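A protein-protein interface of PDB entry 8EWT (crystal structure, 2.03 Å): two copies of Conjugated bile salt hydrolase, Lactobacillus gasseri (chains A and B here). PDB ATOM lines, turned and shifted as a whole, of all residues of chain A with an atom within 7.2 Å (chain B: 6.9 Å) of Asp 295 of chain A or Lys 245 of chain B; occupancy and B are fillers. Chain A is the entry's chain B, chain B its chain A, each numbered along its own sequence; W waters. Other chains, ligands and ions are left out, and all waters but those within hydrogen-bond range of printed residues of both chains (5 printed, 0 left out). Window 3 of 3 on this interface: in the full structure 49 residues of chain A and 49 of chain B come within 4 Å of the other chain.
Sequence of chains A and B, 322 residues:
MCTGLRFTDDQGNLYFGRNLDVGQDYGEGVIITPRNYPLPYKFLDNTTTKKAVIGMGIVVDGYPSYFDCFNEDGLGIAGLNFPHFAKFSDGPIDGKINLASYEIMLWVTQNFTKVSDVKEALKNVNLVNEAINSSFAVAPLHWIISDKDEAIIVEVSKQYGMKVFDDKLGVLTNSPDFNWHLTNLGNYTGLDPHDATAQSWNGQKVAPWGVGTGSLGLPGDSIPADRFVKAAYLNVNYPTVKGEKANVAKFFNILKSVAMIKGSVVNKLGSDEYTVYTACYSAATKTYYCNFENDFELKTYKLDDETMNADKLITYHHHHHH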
ATOM      1  N   LYS A 256     -15.041   1.240  -6.570  1.00  0.00           N
ATOM      2  CA  LYS A 256     -13.649   1.056  -6.166  1.00  0.00           C
ATOM      3  C   LYS A 256     -13.545   0.318  -4.842  1.00  0.00           C
ATOM      4  O   LYS A 256     -12.516  -0.301  -4.567  1.00  0.00           O
ATOM      5  CB  LYS A 256     -12.918   2.397  -6.079  1.00  0.00           C
ATOM      6  CG  LYS A 256     -12.743   3.063  -7.432  1.00  0.00           C
ATOM      7  CD  LYS A 256     -12.046   2.144  -8.408  1.00  0.00           C
ATOM      8  CE  LYS A 256     -11.472   2.924  -9.574  1.00  0.00           C
ATOM      9  NZ  LYS A 256     -11.011   2.020 -10.653  1.00  0.00           N
ATOM     10  N   VAL A 276      -9.544  -3.846 -14.429  1.00  0.00           N
ATOM     11  CA  VAL A 276      -8.735  -3.084 -15.380  1.00  0.00           C
ATOM     12  C   VAL A 276      -9.356  -1.727 -15.672  1.00  0.00           C
ATOM     13  O   VAL A 276      -8.637  -0.780 -16.013  1.00  0.00           O
ATOM     14  CB  VAL A 276      -8.513  -3.860 -16.694  1.00  0.00           C
ATOM     15  CG1 VAL A 276      -7.826  -5.206 -16.418  1.00  0.00           C
ATOM     16  CG2 VAL A 276      -9.820  -4.046 -17.436  1.00  0.00           C
ATOM     17  N   CYS A 290     -14.602   7.003 -17.175  1.00  0.00           N
ATOM     18  CA  CYS A 290     -13.911   5.784 -16.759  1.00  0.00           C
ATOM     19  C   CYS A 290     -12.528   6.125 -16.230  1.00  0.00           C
ATOM     20  O   CYS A 290     -11.995   7.203 -16.494  1.00  0.00           O
ATOM     21  CB  CYS A 290     -13.798   4.766 -17.897  1.00  0.00           C
ATOM     22  SG  CYS A 290     -12.866   5.317 -19.329  1.00  0.00           S
ATOM     23  N   ASN A 291     -11.950   5.192 -15.464  1.00  0.00           N
ATOM     24  CA  ASN A 291     -10.517   5.222 -15.198  1.00  0.00           C
ATOM     25  C   ASN A 291      -9.978   3.793 -15.238  1.00  0.00           C
ATOM     26  O   ASN A 291     -10.709   2.835 -15.518  1.00  0.00           O
ATOM     27  CB  ASN A 291     -10.196   5.995 -13.898  1.00  0.00           C
ATOM     28  CG  ASN A 291     -10.462   5.209 -12.629  1.00  0.00           C
ATOM     29  OD1 ASN A 291     -11.014   4.112 -12.653  1.00  0.00           O
ATOM     30  ND2 ASN A 291     -10.055   5.783 -11.493  1.00  0.00           N
ATOM     31  N   PHE A 292      -8.678   3.655 -14.997  1.00  0.00           N
ATOM     32  CA  PHE A 292      -7.960   2.425 -15.289  1.00  0.00           C
ATOM     33  C   PHE A 292      -7.058   2.033 -14.127  1.00  0.00           C
ATOM     34  O   PHE A 292      -6.699   2.859 -13.277  1.00  0.00           O
ATOM     35  CB  PHE A 292      -7.147   2.586 -16.580  1.00  0.00           C
ATOM     36  CG  PHE A 292      -7.994   2.931 -17.758  1.00  0.00           C
ATOM     37  CD1 PHE A 292      -8.831   1.988 -18.319  1.00  0.00           C
ATOM     38  CD2 PHE A 292      -7.995   4.205 -18.277  1.00  0.00           C
ATOM     39  CE1 PHE A 292      -9.647   2.314 -19.397  1.00  0.00           C
ATOM     40  CE2 PHE A 292      -8.805   4.532 -19.349  1.00  0.00           C
ATOM     41  CZ  PHE A 292      -9.634   3.588 -19.898  1.00  0.00           C
ATOM     42  N   GLU A 293      -6.695   0.742 -14.097  1.00  0.00           N
ATOM     43  CA  GLU A 293      -5.833   0.271 -13.022  1.00  0.00           C
ATOM     44  C   GLU A 293      -4.528   1.062 -12.971  1.00  0.00           C
ATOM     45  O   GLU A 293      -4.016   1.351 -11.881  1.00  0.00           O
ATOM     46  CB  GLU A 293      -5.546  -1.225 -13.163  1.00  0.00           C
ATOM     47  CG  GLU A 293      -4.698  -1.771 -11.996  1.00  0.00           C
ATOM     48  CD  GLU A 293      -3.209  -1.618 -12.242  1.00  0.00           C
ATOM     49  OE1 GLU A 293      -2.820  -1.558 -13.429  1.00  0.00           O
ATOM     50  OE2 GLU A 293      -2.426  -1.539 -11.265  1.00  0.00           O
ATOM     51  N   ASN A 294      -3.972   1.435 -14.127  1.00  0.00           N
ATOM     52  CA  ASN A 294      -2.706   2.167 -14.131  1.00  0.00           C
ATOM     53  C   ASN A 294      -2.853   3.654 -14.452  1.00  0.00           C
ATOM     54  O   ASN A 294      -1.844   4.321 -14.690  1.00  0.00           O
ATOM     55  CB  ASN A 294      -1.714   1.527 -15.107  1.00  0.00           C
ATOM     56  CG  ASN A 294      -2.244   1.462 -16.526  1.00  0.00           C
ATOM     57  OD1 ASN A 294      -3.293   2.022 -16.839  1.00  0.00           O
ATOM     58  ND2 ASN A 294      -1.522   0.765 -17.394  1.00  0.00           N
ATOM     59  N   ASP A 295      -4.067   4.198 -14.450  1.00  0.00           N
ATOM     60  CA  ASP A 295      -4.249   5.607 -14.815  1.00  0.00           C
ATOM     61  C   ASP A 295      -5.538   6.074 -14.144  1.00  0.00           C
ATOM     62  O   ASP A 295      -6.632   5.820 -14.659  1.00  0.00           O
ATOM     63  CB  ASP A 295      -4.286   5.758 -16.332  1.00  0.00           C
ATOM     64  CG  ASP A 295      -4.302   7.214 -16.811  1.00  0.00           C
ATOM     65  OD1 ASP A 295      -4.506   8.167 -16.022  1.00  0.00           O
ATOM     66  OD2 ASP A 295      -4.130   7.398 -18.030  1.00  0.00           O
ATOM     67  N   PHE A 296      -5.400   6.752 -12.994  1.00  0.00           N
ATOM     68  CA  PHE A 296      -6.521   6.953 -12.080  1.00  0.00           C
ATOM     69  C   PHE A 296      -7.376   8.182 -12.386  1.00  0.00           C
ATOM     70  O   PHE A 296      -8.526   8.233 -11.932  1.00  0.00           O
ATOM     71  CB  PHE A 296      -6.026   7.047 -10.622  1.00  0.00           C
ATOM     72  CG  PHE A 296      -7.087   6.694  -9.606  1.00  0.00           C
ATOM     73  CD1 PHE A 296      -7.409   5.371  -9.352  1.00  0.00           C
ATOM     74  CD2 PHE A 296      -7.778   7.692  -8.926  1.00  0.00           C
ATOM     75  CE1 PHE A 296      -8.393   5.053  -8.439  1.00  0.00           C
ATOM     76  CE2 PHE A 296      -8.762   7.383  -8.009  1.00  0.00           C
ATOM     77  CZ  PHE A 296      -9.084   6.061  -7.772  1.00  0.00           C
ATOM     78  N   GLU A 297      -6.863   9.162 -13.133  1.00  0.00           N
ATOM     79  CA  GLU A 297      -7.645  10.356 -13.447  1.00  0.00           C
ATOM     80  C   GLU A 297      -8.839  10.000 -14.328  1.00  0.00           C
ATOM     81  O   GLU A 297      -8.715   9.225 -15.279  1.00  0.00           O
ATOM     82  CB  GLU A 297      -6.772  11.401 -14.150  1.00  0.00           C
ATOM     83  N   LEU A 298     -10.007  10.563 -14.006  1.00  0.00           N
ATOM     84  CA  LEU A 298     -11.221  10.247 -14.762  1.00  0.00           C
ATOM     85  C   LEU A 298     -11.129  10.768 -16.189  1.00  0.00           C
ATOM     86  O   LEU A 298     -10.857  11.953 -16.417  1.00  0.00           O
ATOM     87  CB  LEU A 298     -12.458  10.839 -14.084  1.00  0.00           C
ATOM     88  CG  LEU A 298     -12.928  10.264 -12.752  1.00  0.00           C
ATOM     89  CD1 LEU A 298     -14.341  10.716 -12.497  1.00  0.00           C
ATOM     90  CD2 LEU A 298     -12.878   8.753 -12.772  1.00  0.00           C
ATOM     91  N   LYS A 299     -11.360   9.880 -17.152  1.00  0.00           N
ATOM     92  CA  LYS A 299     -11.504  10.232 -18.557  1.00  0.00           C
ATOM     93  C   LYS A 299     -12.986  10.358 -18.891  1.00  0.00           C
ATOM     94  O   LYS A 299     -13.829   9.694 -18.279  1.00  0.00           O
ATOM     95  CB  LYS A 299     -10.849   9.183 -19.456  1.00  0.00           C
ATOM     96  CG  LYS A 299      -9.327   9.085 -19.279  1.00  0.00           C
ATOM     97  CD  LYS A 299      -8.959   8.004 -18.285  1.00  0.00           C
ATOM     98  CE  LYS A 299      -7.449   7.783 -18.184  1.00  0.00           C
ATOM     99  NZ  LYS A 299      -6.675   8.947 -17.660  1.00  0.00           N
ATOM    100  N   HIS A 319      -6.483   1.432 -24.578  1.00  0.00           N
ATOM    101  CA  HIS A 319      -5.649   1.754 -23.432  1.00  0.00           C
ATOM    102  C   HIS A 319      -4.848   0.521 -23.054  1.00  0.00           C
ATOM    103  O   HIS A 319      -5.420  -0.529 -22.743  1.00  0.00           O
ATOM    104  CB  HIS A 319      -6.499   2.225 -22.252  1.00  0.00           C
ATOM    105  CG  HIS A 319      -5.700   2.445 -21.006  1.00  0.00           C
ATOM    106  ND1 HIS A 319      -5.310   3.700 -20.584  1.00  0.00           N
ATOM    107  CD2 HIS A 319      -5.177   1.569 -20.117  1.00  0.00           C
ATOM    108  CE1 HIS A 319      -4.592   3.586 -19.479  1.00  0.00           C
ATOM    109  NE2 HIS A 319      -4.495   2.303 -19.176  1.00  0.00           N
ATOM    110  N   TYR B  15       5.760   6.766  -2.483  1.00  0.00           N
ATOM    111  CA  TYR B  15       4.350   7.131  -2.619  1.00  0.00           C
ATOM    112  C   TYR B  15       3.696   6.896  -1.263  1.00  0.00           C
ATOM    113  O   TYR B  15       3.661   5.758  -0.786  1.00  0.00           O
ATOM    114  CB  TYR B  15       3.677   6.309  -3.733  1.00  0.00           C
ATOM    115  CG  TYR B  15       4.249   6.686  -5.081  1.00  0.00           C
ATOM    116  CD1 TYR B  15       5.397   6.070  -5.574  1.00  0.00           C
ATOM    117  CD2 TYR B  15       3.681   7.715  -5.828  1.00  0.00           C
ATOM    118  CE1 TYR B  15       5.956   6.467  -6.791  1.00  0.00           C
ATOM    119  CE2 TYR B  15       4.235   8.120  -7.034  1.00  0.00           C
ATOM    120  CZ  TYR B  15       5.357   7.494  -7.513  1.00  0.00           C
ATOM    121  OH  TYR B  15       5.892   7.913  -8.718  1.00  0.00           O
ATOM    122  N   VAL B 241       5.244  -1.260  -9.558  1.00  0.00           N
ATOM    123  CA  VAL B 241       4.885  -0.764 -10.880  1.00  0.00           C
ATOM    124  C   VAL B 241       5.831   0.377 -11.272  1.00  0.00           C
ATOM    125  O   VAL B 241       6.570   0.915 -10.453  1.00  0.00           O
ATOM    126  CB  VAL B 241       3.408  -0.321 -10.955  1.00  0.00           C
ATOM    127  CG1 VAL B 241       2.489  -1.508 -10.653  1.00  0.00           C
ATOM    128  CG2 VAL B 241       3.142   0.817  -9.981  1.00  0.00           C
ATOM    129  N   LYS B 242       5.788   0.746 -12.549  1.00  0.00           N
ATOM    130  CA  LYS B 242       6.743   1.679 -13.134  1.00  0.00           C
ATOM    131  C   LYS B 242       6.052   2.995 -13.485  1.00  0.00           C
ATOM    132  O   LYS B 242       4.977   2.990 -14.091  1.00  0.00           O
ATOM    133  CB  LYS B 242       7.390   1.058 -14.378  1.00  0.00           C
ATOM    134  N   GLY B 243       6.654   4.115 -13.077  1.00  0.00           N
ATOM    135  CA  GLY B 243       6.218   5.426 -13.517  1.00  0.00           C
ATOM    136  C   GLY B 243       5.203   6.086 -12.592  1.00  0.00           C
ATOM    137  O   GLY B 243       4.498   5.439 -11.815  1.00  0.00           O
ATOM    138  N   GLU B 244       5.089   7.408 -12.750  1.00  0.00           N
ATOM    139  CA  GLU B 244       4.275   8.228 -11.854  1.00  0.00           C
ATOM    140  C   GLU B 244       2.790   7.894 -11.963  1.00  0.00           C
ATOM    141  O   GLU B 244       2.097   7.765 -10.945  1.00  0.00           O
ATOM    142  CB  GLU B 244       4.507   9.713 -12.158  1.00  0.00           C
ATOM    143  CG  GLU B 244       3.641  10.677 -11.353  1.00  0.00           C
ATOM    144  CD  GLU B 244       4.262  11.065 -10.011  1.00  0.00           C
ATOM    145  OE1 GLU B 244       5.271  10.449  -9.598  1.00  0.00           O
ATOM    146  OE2 GLU B 244       3.730  11.981  -9.353  1.00  0.00           O
ATOM    147  N   LYS B 245       2.272   7.783 -13.185  1.00  0.00           N
ATOM    148  CA  LYS B 245       0.839   7.559 -13.340  1.00  0.00           C
ATOM    149  C   LYS B 245       0.435   6.218 -12.747  1.00  0.00           C
ATOM    150  O   LYS B 245      -0.534   6.128 -11.984  1.00  0.00           O
ATOM    151  CB  LYS B 245       0.452   7.640 -14.816  1.00  0.00           C
ATOM    152  CG  LYS B 245      -0.388   8.848 -15.168  1.00  0.00           C
ATOM    153  CD  LYS B 245      -0.200   9.246 -16.614  1.00  0.00           C
ATOM    154  CE  LYS B 245      -1.187   8.527 -17.501  1.00  0.00           C
ATOM    155  N   ALA B 246       1.194   5.165 -13.066  1.00  0.00           N
ATOM    156  CA  ALA B 246       0.865   3.828 -12.589  1.00  0.00           C
ATOM    157  C   ALA B 246       0.967   3.732 -11.070  1.00  0.00           C
ATOM    158  O   ALA B 246       0.187   3.014 -10.430  1.00  0.00           O
ATOM    159  CB  ALA B 246       1.783   2.800 -13.256  1.00  0.00           C
ATOM    160  N   ASN B 247       1.933   4.431 -10.472  1.00  0.00           N
ATOM    161  CA  ASN B 247       2.131   4.311  -9.032  1.00  0.00           C
ATOM    162  C   ASN B 247       1.074   5.091  -8.263  1.00  0.00           C
ATOM    163  O   ASN B 247       0.560   4.610  -7.242  1.00  0.00           O
ATOM    164  CB  ASN B 247       3.539   4.774  -8.652  1.00  0.00           C
ATOM    165  CG  ASN B 247       4.574   3.662  -8.790  1.00  0.00           C
ATOM    166  OD1 ASN B 247       4.752   2.849  -7.883  1.00  0.00           O
ATOM    167  ND2 ASN B 247       5.231   3.603  -9.935  1.00  0.00           N
ATOM    168  N   VAL B 248       0.727   6.284  -8.743  1.00  0.00           N
ATOM    169  CA  VAL B 248      -0.348   7.041  -8.114  1.00  0.00           C
ATOM    170  C   VAL B 248      -1.659   6.262  -8.200  1.00  0.00           C
ATOM    171  O   VAL B 248      -2.446   6.218  -7.241  1.00  0.00           O
ATOM    172  CB  VAL B 248      -0.449   8.434  -8.762  1.00  0.00           C
ATOM    173  CG1 VAL B 248      -1.685   9.156  -8.280  1.00  0.00           C
ATOM    174  CG2 VAL B 248       0.807   9.252  -8.454  1.00  0.00           C
ATOM    175  N   ALA B 249      -1.902   5.603  -9.336  1.00  0.00           N
ATOM    176  CA  ALA B 249      -3.152   4.870  -9.484  1.00  0.00           C
ATOM    177  C   ALA B 249      -3.190   3.677  -8.542  1.00  0.00           C
ATOM    178  O   ALA B 249      -4.218   3.406  -7.912  1.00  0.00           O
ATOM    179  CB  ALA B 249      -3.331   4.434 -10.942  1.00  0.00           C
ATOM    180  N   LYS B 250      -2.065   2.969  -8.424  1.00  0.00           N
ATOM    181  CA  LYS B 250      -1.950   1.856  -7.483  1.00  0.00           C
ATOM    182  C   LYS B 250      -2.261   2.308  -6.061  1.00  0.00           C
ATOM    183  O   LYS B 250      -2.989   1.628  -5.322  1.00  0.00           O
ATOM    184  CB  LYS B 250      -0.532   1.268  -7.564  1.00  0.00           C
ATOM    185  CG  LYS B 250      -0.083   0.509  -6.322  1.00  0.00           C
ATOM    186  CD  LYS B 250       1.328  -0.009  -6.473  1.00  0.00           C
ATOM    187  CE  LYS B 250       1.781  -0.752  -5.234  1.00  0.00           C
ATOM    188  NZ  LYS B 250       3.157  -1.303  -5.455  1.00  0.00           N
ATOM    189  N   ASN B 253      -5.976   2.931  -5.894  1.00  0.00           N
ATOM    190  CA  ASN B 253      -6.623   1.615  -5.958  1.00  0.00           C
ATOM    191  C   ASN B 253      -6.668   0.952  -4.583  1.00  0.00           C
ATOM    192  O   ASN B 253      -7.713   0.450  -4.148  1.00  0.00           O
ATOM    193  CB  ASN B 253      -5.880   0.708  -6.943  1.00  0.00           C
ATOM    194  CG  ASN B 253      -6.047   1.141  -8.384  1.00  0.00           C
ATOM    195  OD1 ASN B 253      -7.014   1.808  -8.732  1.00  0.00           O
ATOM    196  ND2 ASN B 253      -5.108   0.751  -9.232  1.00  0.00           N
ATOM    197  N   TYR B 289      -1.412  14.678  -4.328  1.00  0.00           N
ATOM    198  CA  TYR B 289      -2.647  14.333  -5.032  1.00  0.00           C
ATOM    199  C   TYR B 289      -3.776  14.096  -4.043  1.00  0.00           C
ATOM    200  O   TYR B 289      -3.555  13.487  -2.997  1.00  0.00           O
ATOM    201  CB  TYR B 289      -2.481  13.049  -5.846  1.00  0.00           C
ATOM    202  CG  TYR B 289      -1.419  13.060  -6.926  1.00  0.00           C
ATOM    203  CD1 TYR B 289      -0.077  12.834  -6.616  1.00  0.00           C
ATOM    204  CD2 TYR B 289      -1.766  13.248  -8.273  1.00  0.00           C
ATOM    205  CE1 TYR B 289       0.892  12.819  -7.604  1.00  0.00           C
ATOM    206  CE2 TYR B 289      -0.798  13.233  -9.272  1.00  0.00           C
ATOM    207  CZ  TYR B 289       0.527  13.015  -8.930  1.00  0.00           C
ATOM    208  OH  TYR B 289       1.499  13.000  -9.911  1.00  0.00           O
HETATM  209  O   HOH W   1      -9.304  -0.062  -8.611  1.00  0.00           O
HETATM  210  O   HOH W   2      -2.958   7.771 -11.938  1.00  0.00           O
HETATM  211  O   HOH W   3      -8.243   2.362 -10.927  1.00  0.00           O
HETATM  212  O   HOH W   4      -0.535   0.590 -11.587  1.00  0.00           O
HETATM  213  O   HOH W   5     -10.022   0.277  -5.861  1.00  0.00           O
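The side-chain amide nitrogen (ND2) of Asn 253 of chain B lies within hydrogen-bond range of the backbone carbonyl oxygen (O) of Glu 293 of chain A, at 2.9 Å.
O of Ala 249 of chain B sits close to ND2 of Asn 253 of chain B. The side-chain amide oxygen of Asn 294 of chain A is in hydrogen-bond range of a ring nitrogen (NE2) of His 319 of chain A (2.6 Å). O of Val 276 of chain A is in hydrogen-bond range of N of Glu 293 of chain A, 3.1 Å away. OD1 of Asp 295 of chain A lies within salt-bridge range of NZ of Lys 299 of chain A. O of Phe 296 of chain A sits at hydrogen-bond distance from ND2 of Asn 291 of chain A (2.9 Å).
O of Glu 293 of chain A touches CB of Ala 249 of chain B, at 3.3 Å. Asn 294 of chain A touches Lys 245 of chain B. Ala 246 of chain B touches Asn 294 of chain A. Asn 294 of chain A touches Ala 249 of chain B. Asp 295 of chain A touches Lys 245 of chain B (OD2 to CE, 3.2 Å). N of Asp 295 of chain A touches CB of Ala 249 of chain B, 3.6 Å away. Phe 296 of chain A touches Ala 249 of chain B (N to CB, 3.7 Å). Phe 296 of chain A touches Asn 253 of chain B (CE1 to OD1, 3.5 Å).
Asn 291 of chain A touches none of the printed residues of chain B. Of the printed residues of chain B, Asn 294 of chain A touches Lys 245 (3.5 Å), Ala 246 (3.5 Å) and Ala 249 (3.6 Å). Of chain B, only Lys 245 and Ala 249 come within 4 Å of Asp 295 of chain A. Of the printed residues of chain A, Ala 249 of chain B touches Glu 293 (3.3 Å), Asn 294 (3.6 Å), Asp 295 (3.6 Å) and Phe 296 (3.7 Å). Printed residues of chain A within 4 Å of Asn 253 of chain B: Glu 293 and Phe 296. The nearest residue of chain B that does not touch Asp 295 of chain A is Ala 246 of chain B (5.3 Å). The nearest printed residue of chain B that does not touch Glu 293 of chain A is Lys 250 of chain B (4.3 Å).
Of the 13 printed residues of chain B, 4 touch a printed residue of chain A. Of the 13 printed residues of chain A, 4 touch a printed residue of chain B. Among the printed residues, no Asp or Glu carboxylate lies within 4 Å of a Lys or Arg side-chain nitrogen of the other chain.
No position is printed for both chains. Of the 9 pairs that touch across the chains among the printed residues, none has its exchanged pair printed and touching as well.
Water W3 lies within hydrogen-bond range of the side-chain amide oxygen (OD1) of Asn 253 of chain B (2.6 Å), the side-chain amino group (NZ) of Lys 256 of chain A (2.8 Å) and the backbone carbonyl oxygen (O) of Phe 292 of chain A (2.9 Å). Water W4 bridges the backbone carbonyl oxygen (O) of Ala 246 of chain B (2.8 Å) and the side-chain carboxylate (OE2) of Glu 293 of chain A (2.9 Å). Water W2 bridges the backbone NH of Phe 296 of chain A and the backbone carbonyl oxygen of Lys 245 of chain B. Water W5 lies within hydrogen-bond range of O of Lys 256 of chain A (2.9 Å) and O of Asn 253 of chain B (2.9 Å). Water W1 bridges OD1 of Asn 253 of chain B (3.0 Å) and NZ of Lys 256 of chain A (3.4 Å).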
